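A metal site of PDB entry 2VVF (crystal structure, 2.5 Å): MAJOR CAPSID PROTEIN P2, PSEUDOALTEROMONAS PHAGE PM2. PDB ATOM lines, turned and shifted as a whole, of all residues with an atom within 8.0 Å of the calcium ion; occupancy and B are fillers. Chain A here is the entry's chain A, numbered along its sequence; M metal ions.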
ATOM      1  N   THR A  28      16.587  25.658  28.187  1.00  0.00           N
ATOM      2  CA  THR A  28      15.497  26.584  28.477  1.00  0.00           C
ATOM      3  C   THR A  28      15.926  28.020  28.192  1.00  0.00           C
ATOM      4  O   THR A  28      16.998  28.453  28.619  1.00  0.00           O
ATOM      5  CB  THR A  28      15.017  26.437  29.925  1.00  0.00           C
ATOM      6  OG1 THR A  28      14.398  25.160  30.103  1.00  0.00           O
ATOM      7  CG2 THR A  28      14.032  27.538  30.278  1.00  0.00           C
ATOM      8  N   TYR A  29      15.085  28.762  27.477  1.00  0.00           N
ATOM      9  CA  TYR A  29      15.360  30.160  27.165  1.00  0.00           C
ATOM     10  C   TYR A  29      14.543  31.066  28.080  1.00  0.00           C
ATOM     11  O   TYR A  29      13.324  31.161  27.946  1.00  0.00           O
ATOM     12  CB  TYR A  29      15.012  30.462  25.702  1.00  0.00           C
ATOM     13  CG  TYR A  29      15.913  29.766  24.702  1.00  0.00           C
ATOM     14  CD1 TYR A  29      17.103  30.362  24.277  1.00  0.00           C
ATOM     15  CD2 TYR A  29      15.584  28.521  24.196  1.00  0.00           C
ATOM     16  CE1 TYR A  29      17.927  29.720  23.366  1.00  0.00           C
ATOM     17  CE2 TYR A  29      16.408  27.879  23.285  1.00  0.00           C
ATOM     18  CZ  TYR A  29      17.575  28.486  22.871  1.00  0.00           C
ATOM     19  OH  TYR A  29      18.398  27.857  21.966  1.00  0.00           O
ATOM     20  N   PHE A  85      10.580  35.720  28.490  1.00  0.00           N
ATOM     21  CA  PHE A  85       9.742  34.535  28.653  1.00  0.00           C
ATOM     22  C   PHE A  85       9.463  34.373  30.131  1.00  0.00           C
ATOM     23  O   PHE A  85       8.320  34.183  30.551  1.00  0.00           O
ATOM     24  CB  PHE A  85      10.426  33.312  28.053  1.00  0.00           C
ATOM     25  CG  PHE A  85      10.645  33.412  26.575  1.00  0.00           C
ATOM     26  CD1 PHE A  85       9.579  33.375  25.702  1.00  0.00           C
ATOM     27  CD2 PHE A  85      11.909  33.648  26.065  1.00  0.00           C
ATOM     28  CE1 PHE A  85       9.763  33.506  24.336  1.00  0.00           C
ATOM     29  CE2 PHE A  85      12.114  33.786  24.702  1.00  0.00           C
ATOM     30  CZ  PHE A  85      11.039  33.713  23.844  1.00  0.00           C
ATOM     31  N   VAL A  86      10.511  34.520  30.936  1.00  0.00           N
ATOM     32  CA  VAL A  86      10.374  34.487  32.384  1.00  0.00           C
ATOM     33  C   VAL A  86       9.766  35.827  32.769  1.00  0.00           C
ATOM     34  O   VAL A  86      10.258  36.880  32.362  1.00  0.00           O
ATOM     35  CB  VAL A  86      11.744  34.286  33.068  1.00  0.00           C
ATOM     36  CG1 VAL A  86      11.688  34.709  34.521  1.00  0.00           C
ATOM     37  CG2 VAL A  86      12.204  32.847  32.927  1.00  0.00           C
ATOM     38  N   GLN A 101       8.029  33.063  38.556  1.00  0.00           N
ATOM     39  CA  GLN A 101       8.565  33.830  37.428  1.00  0.00           C
ATOM     40  C   GLN A 101       9.218  32.919  36.400  1.00  0.00           C
ATOM     41  O   GLN A 101       8.974  33.045  35.198  1.00  0.00           O
ATOM     42  CB  GLN A 101       9.583  34.857  37.928  1.00  0.00           C
ATOM     43  CG  GLN A 101       9.080  35.777  39.018  1.00  0.00           C
ATOM     44  CD  GLN A 101      10.205  36.424  39.795  1.00  0.00           C
ATOM     45  OE1 GLN A 101      11.374  36.244  39.487  1.00  0.00           O
ATOM     46  NE2 GLN A 101       9.842  37.187  40.827  1.00  0.00           N
ATOM     47  N   ARG A 102      10.058  32.006  36.876  1.00  0.00           N
ATOM     48  CA  ARG A 102      10.773  31.074  36.001  1.00  0.00           C
ATOM     49  C   ARG A 102       9.829  30.080  35.325  1.00  0.00           C
ATOM     50  O   ARG A 102      10.175  29.479  34.302  1.00  0.00           O
ATOM     51  CB  ARG A 102      11.856  30.319  36.781  1.00  0.00           C
ATOM     52  CG  ARG A 102      12.850  31.229  37.499  1.00  0.00           C
ATOM     53  CD  ARG A 102      13.686  30.445  38.495  1.00  0.00           C
ATOM     54  NE  ARG A 102      14.966  31.092  38.757  1.00  0.00           N
ATOM     55  CZ  ARG A 102      15.800  30.734  39.713  1.00  0.00           C
ATOM     56  NH1 ARG A 102      16.951  31.377  39.883  1.00  0.00           N
ATOM     57  NH2 ARG A 102      15.484  29.732  40.524  1.00  0.00           N
ATOM     58  N   MET A 103       8.656  29.890  35.896  1.00  0.00           N
ATOM     59  CA  MET A 103       7.677  28.954  35.343  1.00  0.00           C
ATOM     60  C   MET A 103       7.212  29.330  33.937  1.00  0.00           C
ATOM     61  O   MET A 103       6.569  28.535  33.255  1.00  0.00           O
ATOM     62  CB  MET A 103       6.477  28.821  36.290  1.00  0.00           C
ATOM     63  CG  MET A 103       5.128  28.956  35.620  1.00  0.00           C
ATOM     64  SD  MET A 103       3.764  28.722  36.795  1.00  0.00           S
ATOM     65  CE  MET A 103       2.604  29.946  36.207  1.00  0.00           C
ATOM     66  N   PHE A 104       7.559  30.541  33.506  1.00  0.00           N
ATOM     67  CA  PHE A 104       7.171  31.020  32.188  1.00  0.00           C
ATOM     68  C   PHE A 104       8.294  30.887  31.160  1.00  0.00           C
ATOM     69  O   PHE A 104       8.103  31.186  29.983  1.00  0.00           O
ATOM     70  CB  PHE A 104       6.695  32.466  32.253  1.00  0.00           C
ATOM     71  CG  PHE A 104       5.364  32.625  32.935  1.00  0.00           C
ATOM     72  CD1 PHE A 104       4.183  32.574  32.206  1.00  0.00           C
ATOM     73  CD2 PHE A 104       5.284  32.840  34.295  1.00  0.00           C
ATOM     74  CE1 PHE A 104       2.968  32.722  32.824  1.00  0.00           C
ATOM     75  CE2 PHE A 104       4.067  32.993  34.921  1.00  0.00           C
ATOM     76  CZ  PHE A 104       2.898  32.937  34.187  1.00  0.00           C
ATOM     77  N   ALA A 105       9.458  30.437  31.616  1.00  0.00           N
ATOM     78  CA  ALA A 105      10.613  30.277  30.735  1.00  0.00           C
ATOM     79  C   ALA A 105      10.277  29.374  29.554  1.00  0.00           C
ATOM     80  O   ALA A 105       9.457  28.462  29.663  1.00  0.00           O
ATOM     81  CB  ALA A 105      11.808  29.734  31.506  1.00  0.00           C
ATOM     82  N   LEU A 106      10.938  29.622  28.419  1.00  0.00           N
ATOM     83  CA  LEU A 106      10.700  28.838  27.211  1.00  0.00           C
ATOM     84  C   LEU A 106      11.526  27.558  27.169  1.00  0.00           C
ATOM     85  O   LEU A 106      12.627  27.528  26.612  1.00  0.00           O
ATOM     86  CB  LEU A 106      10.976  29.678  25.963  1.00  0.00           C
ATOM     87  CG  LEU A 106      10.854  28.956  24.621  1.00  0.00           C
ATOM     88  CD1 LEU A 106       9.502  28.283  24.499  1.00  0.00           C
ATOM     89  CD2 LEU A 106      11.080  29.937  23.475  1.00  0.00           C
ATOM     90  N   GLY A 107      10.983  26.488  27.752  1.00  0.00           N
ATOM     91  CA  GLY A 107      11.661  25.201  27.740  1.00  0.00           C
ATOM     92  C   GLY A 107      11.532  24.648  26.318  1.00  0.00           C
ATOM     93  O   GLY A 107      10.537  24.905  25.647  1.00  0.00           O
ATOM     94  N   THR A 108      12.536  23.903  25.872  1.00  0.00           N
ATOM     95  CA  THR A 108      12.524  23.357  24.515  1.00  0.00           C
ATOM     96  C   THR A 108      12.561  21.828  24.464  1.00  0.00           C
ATOM     97  O   THR A 108      12.492  21.240  23.384  1.00  0.00           O
ATOM     98  CB  THR A 108      13.625  23.976  23.643  1.00  0.00           C
ATOM     99  OG1 THR A 108      14.909  23.553  24.132  1.00  0.00           O
ATOM    100  CG2 THR A 108      13.547  25.492  23.688  1.00  0.00           C
ATOM    101  N   THR A 139      13.856  22.184  30.025  1.00  0.00           N
ATOM    102  CA  THR A 139      12.547  21.841  30.570  1.00  0.00           C
ATOM    103  C   THR A 139      11.570  21.786  29.401  1.00  0.00           C
ATOM    104  O   THR A 139      11.859  22.328  28.329  1.00  0.00           O
ATOM    105  CB  THR A 139      12.075  22.888  31.611  1.00  0.00           C
ATOM    106  OG1 THR A 139      11.793  24.131  30.948  1.00  0.00           O
ATOM    107  CG2 THR A 139      13.127  23.093  32.675  1.00  0.00           C
ATOM    108  N   ALA A 140      10.423  21.153  29.593  1.00  0.00           N
ATOM    109  CA  ALA A 140       9.416  21.097  28.541  1.00  0.00           C
ATOM    110  C   ALA A 140       8.885  22.512  28.353  1.00  0.00           C
ATOM    111  O   ALA A 140       9.072  23.355  29.234  1.00  0.00           O
ATOM    112  CB  ALA A 140       8.294  20.150  28.932  1.00  0.00           C
ATOM    113  N   PRO A 141       8.239  22.776  27.221  1.00  0.00           N
ATOM    114  CA  PRO A 141       7.680  24.090  26.958  1.00  0.00           C
ATOM    115  C   PRO A 141       6.818  24.513  28.155  1.00  0.00           C
ATOM    116  O   PRO A 141       6.949  25.621  28.668  1.00  0.00           O
ATOM    117  CB  PRO A 141       6.822  23.858  25.723  1.00  0.00           C
ATOM    118  CG  PRO A 141       7.563  22.794  24.975  1.00  0.00           C
ATOM    119  CD  PRO A 141       8.310  21.953  25.995  1.00  0.00           C
ATOM    120  N   SER A 142       5.966  23.601  28.608  1.00  0.00           N
ATOM    121  CA  SER A 142       5.115  23.831  29.773  1.00  0.00           C
ATOM    122  C   SER A 142       4.364  25.160  29.733  1.00  0.00           C
ATOM    123  O   SER A 142       3.877  25.584  28.686  1.00  0.00           O
ATOM    124  CB  SER A 142       5.953  23.720  31.048  1.00  0.00           C
ATOM    125  OG  SER A 142       5.173  23.972  32.200  1.00  0.00           O
ATOM    126  N   TRP A 143       4.231  25.795  30.892  1.00  0.00           N
ATOM    127  CA  TRP A 143       3.524  27.068  31.017  1.00  0.00           C
ATOM    128  C   TRP A 143       4.189  28.175  30.213  1.00  0.00           C
ATOM    129  O   TRP A 143       5.341  28.545  30.476  1.00  0.00           O
ATOM    130  CB  TRP A 143       3.388  27.484  32.484  1.00  0.00           C
ATOM    131  CG  TRP A 143       2.069  27.121  33.082  1.00  0.00           C
ATOM    132  CD1 TRP A 143       1.753  25.962  33.749  1.00  0.00           C
ATOM    133  CD2 TRP A 143       0.856  27.884  33.025  1.00  0.00           C
ATOM    134  NE1 TRP A 143       0.428  25.971  34.115  1.00  0.00           N
ATOM    135  CE2 TRP A 143      -0.141  27.142  33.677  1.00  0.00           C
ATOM    136  CE3 TRP A 143       0.533  29.130  32.486  1.00  0.00           C
ATOM    137  CZ2 TRP A 143      -1.445  27.611  33.822  1.00  0.00           C
ATOM    138  CZ3 TRP A 143      -0.769  29.595  32.622  1.00  0.00           C
ATOM    139  CH2 TRP A 143      -1.740  28.828  33.282  1.00  0.00           C
ATOM    140  N   LEU A 144       3.465  28.722  29.246  1.00  0.00           N
ATOM    141  CA  LEU A 144       3.992  29.789  28.397  1.00  0.00           C
ATOM    142  C   LEU A 144       2.959  30.898  28.208  1.00  0.00           C
ATOM    143  O   LEU A 144       1.759  30.678  28.351  1.00  0.00           O
ATOM    144  CB  LEU A 144       4.356  29.221  27.022  1.00  0.00           C
ATOM    145  CG  LEU A 144       5.825  28.893  26.722  1.00  0.00           C
ATOM    146  CD1 LEU A 144       6.604  28.603  27.984  1.00  0.00           C
ATOM    147  CD2 LEU A 144       5.906  27.717  25.754  1.00  0.00           C
ATOM    148  N   THR A 145       3.443  32.090  27.870  1.00  0.00           N
ATOM    149  CA  THR A 145       2.583  33.230  27.591  1.00  0.00           C
ATOM    150  C   THR A 145       2.292  33.209  26.102  1.00  0.00           C
ATOM    151  O   THR A 145       3.207  33.102  25.287  1.00  0.00           O
ATOM    152  CB  THR A 145       3.243  34.561  27.993  1.00  0.00           C
ATOM    153  OG1 THR A 145       3.409  34.610  29.421  1.00  0.00           O
ATOM    154  CG2 THR A 145       2.391  35.743  27.547  1.00  0.00           C
ATOM    155  N   GLY A 262      -1.088  29.104  29.507  1.00  0.00           N
ATOM    156  CA  GLY A 262      -1.440  27.699  29.640  1.00  0.00           C
ATOM    157  C   GLY A 262      -0.242  26.814  29.327  1.00  0.00           C
ATOM    158  O   GLY A 262       0.772  27.288  28.817  1.00  0.00           O
ATOM    159  N   VAL A 263      -0.347  25.532  29.646  1.00  0.00           N
ATOM    160  CA  VAL A 263       0.685  24.542  29.380  1.00  0.00           C
ATOM    161  C   VAL A 263       0.644  24.270  27.886  1.00  0.00           C
ATOM    162  O   VAL A 263      -0.369  23.821  27.346  1.00  0.00           O
ATOM    163  CB  VAL A 263       0.459  23.233  30.200  1.00  0.00           C
ATOM    164  CG1 VAL A 263       1.456  22.178  29.829  1.00  0.00           C
ATOM    165  CG2 VAL A 263       0.446  23.510  31.698  1.00  0.00           C
ATOM    166  N   TRP A 264       1.760  24.564  27.238  1.00  0.00           N
ATOM    167  CA  TRP A 264       1.856  24.371  25.805  1.00  0.00           C
ATOM    168  C   TRP A 264       1.594  22.923  25.412  1.00  0.00           C
ATOM    169  O   TRP A 264       2.107  21.992  26.030  1.00  0.00           O
ATOM    170  CB  TRP A 264       3.220  24.823  25.292  1.00  0.00           C
ATOM    171  CG  TRP A 264       3.304  24.806  23.795  1.00  0.00           C
ATOM    172  CD1 TRP A 264       2.879  25.774  22.934  1.00  0.00           C
ATOM    173  CD2 TRP A 264       3.816  23.748  22.977  1.00  0.00           C
ATOM    174  NE1 TRP A 264       3.111  25.388  21.630  1.00  0.00           N
ATOM    175  CE2 TRP A 264       3.693  24.152  21.634  1.00  0.00           C
ATOM    176  CE3 TRP A 264       4.388  22.490  23.251  1.00  0.00           C
ATOM    177  CZ2 TRP A 264       4.107  23.351  20.565  1.00  0.00           C
ATOM    178  CZ3 TRP A 264       4.799  21.706  22.196  1.00  0.00           C
ATOM    179  CH2 TRP A 264       4.652  22.133  20.870  1.00  0.00           C
HETATM  180 CA    CA M   1       7.643  27.067  30.749  1.00  0.00          CA
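Merely in contact with the calcium ion: Phe 104 (3.9 Å), Ser 142 (3.8 Å) and Leu 144 (3.3 Å).
The calcium ion is bound by O of Ala 105, O of Pro 141 and O of Trp 143. The calcium ion has three donor atoms within binding distance. Slightly farther from the calcium ion lies the backbone carbonyl oxygen (O) of Met 103 (3.1 Å).
The backbone carbonyl oxygen of Ser 142 sits at hydrogen-bond distance from the backbone NH of Trp 264 (2.8 Å). The backbone NH (N) of Leu 144 is in hydrogen-bond range of the backbone carbonyl oxygen (O) of Gly 262, at 3.1 Å.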
